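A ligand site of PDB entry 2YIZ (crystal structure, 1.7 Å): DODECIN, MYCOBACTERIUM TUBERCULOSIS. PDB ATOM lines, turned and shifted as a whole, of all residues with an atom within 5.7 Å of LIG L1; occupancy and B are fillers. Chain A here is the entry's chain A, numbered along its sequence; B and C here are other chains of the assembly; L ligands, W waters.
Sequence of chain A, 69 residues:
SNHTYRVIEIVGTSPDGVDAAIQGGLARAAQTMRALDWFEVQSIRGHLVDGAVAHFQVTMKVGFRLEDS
CD2 of His 3 touches O9 of LIG L1, at 2.8 Å. Trp 38 touches LIG L1 (CE2 to C5, 3.7 Å). CB of His 47 of chain B touches O1 of LIG L1, at 3.3 Å. Val 11 of chain C touches LIG L1. CD of Gln 57 of chain C touches C9 of LIG L1, 3.4 Å away. Thr 59 of chain C touches LIG L1. Hydrophobic or aromatic side chains within 4 Å of LIG L1: His 3, Tyr 5, Trp 38, His 47 of chain B and Val 11 of chain C. 11 residues have an atom within 4 Å of LIG L1: His 3, Tyr 5, Asp 37, Trp 38, Arg 65, Arg 45 of chain B, His 47 of chain B, Gln 57 of chain B, Val 11 of chain C, Gln 57 of chain C and Thr 59 of chain C.
Water W2 lies within hydrogen-bond range of an oxygen (O8) of LIG L1 (2.7 Å), the side-chain carboxylate of Asp 37 (3.1 Å) and the guanidinium group of Arg 65 (3.1 Å).
N of Val 11 of chain C is in hydrogen-bond range of O of Tyr 5, 2.8 Å away. ND1 of His 47 of chain B is in hydrogen-bond range of O of Asp 37 (3.2 Å). O of Arg 45 of chain B lies within hydrogen-bond range of N of Gln 57 of chain B, at 2.8 Å. The side-chain hydroxyl (OG1) of Thr 13 of chain C lies within hydrogen-bond range of the backbone carbonyl oxygen (O) of His 3 (2.7 Å). The backbone carbonyl oxygen (O) of Ala 35 sits at hydrogen-bond distance from the backbone NH (N) of Arg 65. The backbone NH of Gln 57 of chain C lies within hydrogen-bond range of the backbone carbonyl oxygen of Arg 45 of chain C (2.8 Å). The backbone carbonyl oxygen (O) of Ser 43 of chain C is in hydrogen-bond range of the backbone NH (N) of Thr 59 of chain C, 3.0 Å away.
OH of Tyr 5 sits at hydrogen-bond distance from O9 of LIG L1 (2.4 Å). O3 of LIG L1 lies within hydrogen-bond range of O of Asp 37 (3.3 Å). An oxygen (O8) of LIG L1 sits close to the side-chain carboxylate (OD2) of Asp 37 (2.6 Å). A nitrogen (N2) of LIG L1 lies within hydrogen-bond range of the side-chain amide oxygen (OE1) of Gln 57 of chain B (2.7 Å). The guanidinium group (NE) of Arg 45 of chain B lies within hydrogen-bond range of an oxygen (O2) of LIG L1, at 2.7 Å. O8 of LIG L1 is in salt-bridge range of NE of Arg 65, at 3.3 Å. OE1 of Gln 57 of chain C sits at hydrogen-bond distance from N2 of LG2 L2 (2.7 Å). O2 of LG2 L2 lies within hydrogen-bond range of NE of Arg 45 of chain C (2.7 Å).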
ATOM      1  N   HIS A   3      15.101   8.658   3.166  1.00  0.00           N
ATOM      2  CA  HIS A   3      14.606   8.410   1.826  1.00  0.00           C
ATOM      3  C   HIS A   3      15.631   8.861   0.783  1.00  0.00           C
ATOM      4  O   HIS A   3      16.429   9.744   1.051  1.00  0.00           O
ATOM      5  CB  HIS A   3      13.317   9.200   1.603  1.00  0.00           C
ATOM      6  CG  HIS A   3      12.221   8.843   2.544  1.00  0.00           C
ATOM      7  ND1 HIS A   3      12.193   7.666   3.236  1.00  0.00           N
ATOM      8  CD2 HIS A   3      11.083   9.513   2.874  1.00  0.00           C
ATOM      9  CE1 HIS A   3      11.092   7.618   3.974  1.00  0.00           C
ATOM     10  NE2 HIS A   3      10.406   8.731   3.775  1.00  0.00           N
ATOM     11  N   TYR A   5      15.677  10.045  -3.389  1.00  0.00           N
ATOM     12  CA  TYR A   5      14.799  10.511  -4.465  1.00  0.00           C
ATOM     13  C   TYR A   5      15.522  10.389  -5.792  1.00  0.00           C
ATOM     14  O   TYR A   5      16.768  10.356  -5.852  1.00  0.00           O
ATOM     15  CB  TYR A   5      14.348  11.957  -4.246  1.00  0.00           C
ATOM     16  CG  TYR A   5      13.724  12.161  -2.894  1.00  0.00           C
ATOM     17  CD1 TYR A   5      14.520  12.297  -1.761  1.00  0.00           C
ATOM     18  CD2 TYR A   5      12.345  12.159  -2.733  1.00  0.00           C
ATOM     19  CE1 TYR A   5      13.970  12.443  -0.505  1.00  0.00           C
ATOM     20  CE2 TYR A   5      11.789  12.311  -1.472  1.00  0.00           C
ATOM     21  CZ  TYR A   5      12.616  12.460  -0.363  1.00  0.00           C
ATOM     22  OH  TYR A   5      12.074  12.607   0.916  1.00  0.00           O
ATOM     23  N   ALA A  35       4.841   8.237  -6.534  1.00  0.00           N
ATOM     24  CA  ALA A  35       5.455   8.963  -5.433  1.00  0.00           C
ATOM     25  C   ALA A  35       6.085  10.262  -5.937  1.00  0.00           C
ATOM     26  O   ALA A  35       7.137  10.683  -5.440  1.00  0.00           O
ATOM     27  CB  ALA A  35       6.495   8.091  -4.714  1.00  0.00           C
ATOM     28  N   ASP A  37       6.826  14.054  -6.050  1.00  0.00           N
ATOM     29  CA  ASP A  37       6.905  14.912  -4.882  1.00  0.00           C
ATOM     30  C   ASP A  37       7.037  16.387  -5.264  1.00  0.00           C
ATOM     31  O   ASP A  37       6.363  17.229  -4.662  1.00  0.00           O
ATOM     32  CB  ASP A  37       8.082  14.517  -3.980  1.00  0.00           C
ATOM     33  CG  ASP A  37       7.753  13.396  -2.982  1.00  0.00           C
ATOM     34  OD1 ASP A  37       6.562  13.154  -2.625  1.00  0.00           O
ATOM     35  OD2 ASP A  37       8.719  12.746  -2.515  1.00  0.00           O
ATOM     36  N   TRP A  38       7.898  16.705  -6.224  1.00  0.00           N
ATOM     37  CA  TRP A  38       8.097  18.130  -6.597  1.00  0.00           C
ATOM     38  C   TRP A  38       8.496  18.262  -8.059  1.00  0.00           C
ATOM     39  O   TRP A  38       8.893  17.301  -8.696  1.00  0.00           O
ATOM     40  CB  TRP A  38       9.105  18.820  -5.693  1.00  0.00           C
ATOM     41  CG  TRP A  38      10.560  18.575  -6.048  1.00  0.00           C
ATOM     42  CD1 TRP A  38      11.332  19.340  -6.865  1.00  0.00           C
ATOM     43  CD2 TRP A  38      11.396  17.464  -5.634  1.00  0.00           C
ATOM     44  NE1 TRP A  38      12.600  18.815  -6.967  1.00  0.00           N
ATOM     45  CE2 TRP A  38      12.660  17.659  -6.225  1.00  0.00           C
ATOM     46  CE3 TRP A  38      11.203  16.368  -4.793  1.00  0.00           C
ATOM     47  CZ2 TRP A  38      13.733  16.778  -6.012  1.00  0.00           C
ATOM     48  CZ3 TRP A  38      12.269  15.486  -4.603  1.00  0.00           C
ATOM     49  CH2 TRP A  38      13.504  15.710  -5.217  1.00  0.00           C
ATOM     50  N   PHE A  39       8.360  19.475  -8.583  1.00  0.00           N
ATOM     51  CA  PHE A  39       8.949  19.817  -9.878  1.00  0.00           C
ATOM     52  C   PHE A  39       9.605  21.186  -9.806  1.00  0.00           C
ATOM     53  O   PHE A  39       9.346  21.992  -8.905  1.00  0.00           O
ATOM     54  CB  PHE A  39       7.925  19.795 -11.007  1.00  0.00           C
ATOM     55  CG  PHE A  39       6.935  20.946 -10.984  1.00  0.00           C
ATOM     56  CD1 PHE A  39       5.786  20.856 -10.223  1.00  0.00           C
ATOM     57  CD2 PHE A  39       7.165  22.109 -11.695  1.00  0.00           C
ATOM     58  CE1 PHE A  39       4.877  21.881 -10.194  1.00  0.00           C
ATOM     59  CE2 PHE A  39       6.242  23.170 -11.651  1.00  0.00           C
ATOM     60  CZ  PHE A  39       5.112  23.037 -10.911  1.00  0.00           C
ATOM     61  N   ARG A  65      10.063   9.871  -4.844  1.00  0.00           N
ATOM     62  CA  ARG A  65      10.685   9.042  -3.868  1.00  0.00           C
ATOM     63  C   ARG A  65      10.927   7.630  -4.397  1.00  0.00           C
ATOM     64  O   ARG A  65       9.981   6.961  -4.864  1.00  0.00           O
ATOM     65  CB  ARG A  65       9.837   8.963  -2.610  1.00  0.00           C
ATOM     66  CG  ARG A  65      10.634   8.368  -1.472  1.00  0.00           C
ATOM     67  CD  ARG A  65       9.865   7.478  -0.614  1.00  0.00           C
ATOM     68  NE  ARG A  65       8.896   8.155   0.224  1.00  0.00           N
ATOM     69  CZ  ARG A  65       7.569   7.964   0.174  1.00  0.00           C
ATOM     70  NH1 ARG A  65       6.992   7.159  -0.732  1.00  0.00           N
ATOM     71  NH2 ARG A  65       6.798   8.603   1.052  1.00  0.00           N
ATOM     72  N   ARG B  45       8.635  26.352  -9.092  1.00  0.00           N
ATOM     73  CA  ARG B  45       8.642  25.007  -8.580  1.00  0.00           C
ATOM     74  C   ARG B  45       7.219  24.654  -8.191  1.00  0.00           C
ATOM     75  O   ARG B  45       6.299  25.477  -8.290  1.00  0.00           O
ATOM     76  CB  ARG B  45       9.571  24.956  -7.360  1.00  0.00           C
ATOM     77  CG  ARG B  45      10.994  25.353  -7.695  1.00  0.00           C
ATOM     78  CD  ARG B  45      11.861  25.581  -6.449  1.00  0.00           C
ATOM     79  NE  ARG B  45      12.207  24.307  -5.865  1.00  0.00           N
ATOM     80  CZ  ARG B  45      13.343  23.637  -6.073  1.00  0.00           C
ATOM     81  NH1 ARG B  45      14.335  24.120  -6.829  1.00  0.00           N
ATOM     82  NH2 ARG B  45      13.494  22.445  -5.490  1.00  0.00           N
ATOM     83  N   GLY B  46       7.001  23.429  -7.733  1.00  0.00           N
ATOM     84  CA  GLY B  46       5.729  23.097  -7.130  1.00  0.00           C
ATOM     85  C   GLY B  46       5.786  21.810  -6.361  1.00  0.00           C
ATOM     86  O   GLY B  46       6.700  20.994  -6.539  1.00  0.00           O
ATOM     87  N   HIS B  47       4.798  21.650  -5.483  1.00  0.00           N
ATOM     88  CA  HIS B  47       4.618  20.464  -4.667  1.00  0.00           C
ATOM     89  C   HIS B  47       3.509  19.631  -5.280  1.00  0.00           C
ATOM     90  O   HIS B  47       2.428  20.146  -5.568  1.00  0.00           O
ATOM     91  CB  HIS B  47       4.238  20.890  -3.255  1.00  0.00           C
ATOM     92  CG  HIS B  47       4.042  19.757  -2.302  1.00  0.00           C
ATOM     93  ND1 HIS B  47       4.866  18.650  -2.274  1.00  0.00           N
ATOM     94  CD2 HIS B  47       3.100  19.548  -1.346  1.00  0.00           C
ATOM     95  CE1 HIS B  47       4.448  17.813  -1.347  1.00  0.00           C
ATOM     96  NE2 HIS B  47       3.380  18.324  -0.772  1.00  0.00           N
ATOM     97  N   GLN B  57       4.841  27.245  -6.730  1.00  0.00           N
ATOM     98  CA  GLN B  57       5.680  28.006  -5.793  1.00  0.00           C
ATOM     99  C   GLN B  57       6.626  28.857  -6.628  1.00  0.00           C
ATOM    100  O   GLN B  57       7.499  28.319  -7.324  1.00  0.00           O
ATOM    101  CB  GLN B  57       6.458  27.078  -4.901  1.00  0.00           C
ATOM    102  CG  GLN B  57       5.603  26.176  -4.051  1.00  0.00           C
ATOM    103  CD  GLN B  57       6.314  24.951  -3.577  1.00  0.00           C
ATOM    104  OE1 GLN B  57       7.256  24.478  -4.201  1.00  0.00           O
ATOM    105  NE2 GLN B  57       5.858  24.395  -2.446  1.00  0.00           N
ATOM    106  N   VAL C  11      18.781  12.180  -5.128  1.00  0.00           N
ATOM    107  CA  VAL C  11      18.988  12.985  -3.944  1.00  0.00           C
ATOM    108  C   VAL C  11      19.155  12.026  -2.774  1.00  0.00           C
ATOM    109  O   VAL C  11      18.245  11.248  -2.502  1.00  0.00           O
ATOM    110  CB  VAL C  11      17.777  13.888  -3.650  1.00  0.00           C
ATOM    111  CG1 VAL C  11      18.106  14.841  -2.480  1.00  0.00           C
ATOM    112  CG2 VAL C  11      17.366  14.704  -4.903  1.00  0.00           C
ATOM    113  N   THR C  13      19.706  11.518   1.380  1.00  0.00           N
ATOM    114  CA  THR C  13      19.347  12.272   2.571  1.00  0.00           C
ATOM    115  C   THR C  13      19.873  11.612   3.830  1.00  0.00           C
ATOM    116  O   THR C  13      20.113  10.387   3.876  1.00  0.00           O
ATOM    117  CB  THR C  13      17.800  12.455   2.740  1.00  0.00           C
ATOM    118  OG1 THR C  13      17.167  11.222   3.129  1.00  0.00           O
ATOM    119  CG2 THR C  13      17.162  12.981   1.451  1.00  0.00           C
ATOM    120  N   SER C  43      23.558  20.223  -5.597  1.00  0.00           N
ATOM    121  CA  SER C  43      23.099  21.128  -4.563  1.00  0.00           C
ATOM    122  C   SER C  43      23.079  20.441  -3.201  1.00  0.00           C
ATOM    123  O   SER C  43      22.990  19.218  -3.108  1.00  0.00           O
ATOM    124  CB  SER C  43      21.700  21.657  -4.861  1.00  0.00           C
ATOM    125  OG  SER C  43      20.759  20.631  -4.874  1.00  0.00           O
ATOM    126  N   ARG C  45      20.869  21.054   0.229  1.00  0.00           N
ATOM    127  CA  ARG C  45      19.695  21.671   0.817  1.00  0.00           C
ATOM    128  C   ARG C  45      19.374  20.915   2.086  1.00  0.00           C
ATOM    129  O   ARG C  45      20.017  19.916   2.432  1.00  0.00           O
ATOM    130  CB  ARG C  45      18.537  21.570  -0.178  1.00  0.00           C
ATOM    131  CG  ARG C  45      18.853  22.271  -1.493  1.00  0.00           C
ATOM    132  CD  ARG C  45      17.836  21.953  -2.607  1.00  0.00           C
ATOM    133  NE  ARG C  45      16.611  22.680  -2.349  1.00  0.00           N
ATOM    134  CZ  ARG C  45      16.259  23.841  -2.894  1.00  0.00           C
ATOM    135  NH1 ARG C  45      17.013  24.449  -3.808  1.00  0.00           N
ATOM    136  NH2 ARG C  45      15.103  24.399  -2.521  1.00  0.00           N
ATOM    137  N   GLN C  57      19.886  17.158   2.402  1.00  0.00           N
ATOM    138  CA  GLN C  57      19.423  16.623   1.123  1.00  0.00           C
ATOM    139  C   GLN C  57      20.445  17.027   0.063  1.00  0.00           C
ATOM    140  O   GLN C  57      20.593  18.213  -0.217  1.00  0.00           O
ATOM    141  CB  GLN C  57      18.066  17.191   0.765  1.00  0.00           C
ATOM    142  CG  GLN C  57      16.991  16.866   1.757  1.00  0.00           C
ATOM    143  CD  GLN C  57      15.828  17.819   1.702  1.00  0.00           C
ATOM    144  OE1 GLN C  57      15.971  18.961   1.309  1.00  0.00           O
ATOM    145  NE2 GLN C  57      14.643  17.349   2.117  1.00  0.00           N
ATOM    146  N   THR C  59      21.707  16.585  -3.720  1.00  0.00           N
ATOM    147  CA  THR C  59      21.367  16.214  -5.099  1.00  0.00           C
ATOM    148  C   THR C  59      22.667  15.931  -5.826  1.00  0.00           C
ATOM    149  O   THR C  59      23.575  16.724  -5.782  1.00  0.00           O
ATOM    150  CB  THR C  59      20.564  17.306  -5.780  1.00  0.00           C
ATOM    151  OG1 THR C  59      19.345  17.551  -5.027  1.00  0.00           O
ATOM    152  CG2 THR C  59      20.191  16.912  -7.250  1.00  0.00           C
HETATM  153  N1  LIG L   1       8.759  20.604  -1.600  1.00  0.00           N
HETATM  154  C1  LIG L   1       8.059  21.669  -2.107  1.00  0.00           C
HETATM  155  O1  LIG L   1       6.931  21.875  -1.688  1.00  0.00           O
HETATM  156  N2  LIG L   1       8.628  22.486  -3.090  1.00  0.00           N
HETATM  157  C2  LIG L   1       9.903  22.240  -3.528  1.00  0.00           C
HETATM  158  O2  LIG L   1      10.405  22.971  -4.400  1.00  0.00           O
HETATM  159  C3  LIG L   1      10.626  21.152  -2.993  1.00  0.00           C
HETATM  160  N3  LIG L   1      11.928  20.874  -3.387  1.00  0.00           N
HETATM  161  C4  LIG L   1      12.627  19.787  -2.857  1.00  0.00           C
HETATM  162  C5  LIG L   1      13.928  19.518  -3.281  1.00  0.00           C
HETATM  163  C6  LIG L   1      14.640  18.430  -2.755  1.00  0.00           C
HETATM  164  C7  LIG L   1      16.028  18.145  -3.227  1.00  0.00           C
HETATM  165  C8  LIG L   1      14.036  17.619  -1.808  1.00  0.00           C
HETATM  166  C9  LIG L   1      14.783  16.447  -1.225  1.00  0.00           C
HETATM  167  C10 LIG L   1      12.747  17.888  -1.375  1.00  0.00           C
HETATM  168  C11 LIG L   1      12.027  18.984  -1.881  1.00  0.00           C
HETATM  169  N4  LIG L   1      10.736  19.280  -1.479  1.00  0.00           N
HETATM  170  C12 LIG L   1      10.039  20.348  -2.022  1.00  0.00           C
HETATM  171  C13 LIG L   1      10.027  18.448  -0.442  1.00  0.00           C
HETATM  172  C14 LIG L   1       9.364  17.293  -1.157  1.00  0.00           C
HETATM  173  O3  LIG L   1       8.413  17.788  -2.083  1.00  0.00           O
HETATM  174  C15 LIG L   1       8.669  16.357  -0.180  1.00  0.00           C
HETATM  175  O4  LIG L   1       7.629  17.056   0.448  1.00  0.00           O
HETATM  176  C16 LIG L   1       9.621  15.797   0.876  1.00  0.00           C
HETATM  177  O5  LIG L   1      10.870  15.428   0.328  1.00  0.00           O
HETATM  178  C17 LIG L   1       9.016  14.579   1.536  1.00  0.00           C
HETATM  179  O6  LIG L   1       8.676  13.625   0.551  1.00  0.00           O
HETATM  180  P1  LIG L   1       8.615  12.048   0.885  1.00  0.00           P
HETATM  181  O7  LIG L   1       7.547  11.846   1.954  1.00  0.00           O
HETATM  182  O8  LIG L   1       8.310  11.305  -0.402  1.00  0.00           O
HETATM  183  O9  LIG L   1       9.925  11.601   1.469  1.00  0.00           O
HETATM  184  N1  LG2 L   2      11.507  20.972   1.524  1.00  0.00           N
HETATM  185  C1  LG2 L   2      12.607  20.176   1.662  1.00  0.00           C
HETATM  186  O1  LG2 L   2      12.515  19.203   2.395  1.00  0.00           O
HETATM  187  N2  LG2 L   2      13.776  20.444   0.974  1.00  0.00           N
HETATM  188  C2  LG2 L   2      13.832  21.531   0.129  1.00  0.00           C
HETATM  189  O2  LG2 L   2      14.873  21.762  -0.485  1.00  0.00           O
HETATM  190  C3  LG2 L   2      12.696  22.365  -0.011  1.00  0.00           C
HETATM  191  N3  LG2 L   2      12.691  23.456  -0.860  1.00  0.00           N
HETATM  192  C4  LG2 L   2      11.565  24.268  -0.967  1.00  0.00           C
HETATM  193  C5  LG2 L   2      11.591  25.385  -1.820  1.00  0.00           C
HETATM  194  C6  LG2 L   2      10.473  26.207  -1.949  1.00  0.00           C
HETATM  195  C7  LG2 L   2      10.531  27.399  -2.860  1.00  0.00           C
HETATM  196  C8  LG2 L   2       9.322  25.922  -1.227  1.00  0.00           C
HETATM  197  C9  LG2 L   2       8.109  26.798  -1.342  1.00  0.00           C
HETATM  198  C10 LG2 L   2       9.289  24.817  -0.377  1.00  0.00           C
HETATM  199  C11 LG2 L   2      10.411  23.971  -0.252  1.00  0.00           C
HETATM  200  N4  LG2 L   2      10.411  22.855   0.569  1.00  0.00           N
HETATM  201  C12 LG2 L   2      11.540  22.074   0.696  1.00  0.00           C
HETATM  202  C13 LG2 L   2       9.195  22.471   1.368  1.00  0.00           C
HETATM  203  C14 LG2 L   2       9.245  23.256   2.668  1.00  0.00           C
HETATM  204  O3  LG2 L   2      10.408  22.885   3.369  1.00  0.00           O
HETATM  205  C15 LG2 L   2       7.997  23.005   3.513  1.00  0.00           C
HETATM  206  O4  LG2 L   2       7.978  21.652   3.906  1.00  0.00           O
HETATM  207  C16 LG2 L   2       6.702  23.347   2.783  1.00  0.00           C
HETATM  208  O5  LG2 L   2       6.815  24.576   2.087  1.00  0.00           O
HETATM  209  C17 LG2 L   2       5.566  23.468   3.787  1.00  0.00           C
HETATM  210  O6  LG2 L   2       5.912  24.437   4.742  1.00  0.00           O
HETATM  211  P1  LG2 L   2       4.793  25.239   5.569  1.00  0.00           P
HETATM  212  O7  LG2 L   2       3.959  24.211   6.320  1.00  0.00           O
HETATM  213  O8  LG2 L   2       5.498  26.215   6.475  1.00  0.00           O
HETATM  214  O9  LG2 L   2       3.881  25.925   4.596  1.00  0.00           O
HETATM  215  O   HOH W   1       5.368  15.288  -0.010  1.00  0.00           O
HETATM  216  O   HOH W   2       6.043  10.353  -1.445  1.00  0.00           O
HETATM  217  O   HOH W   3      17.128  18.550  -6.318  1.00  0.00           O
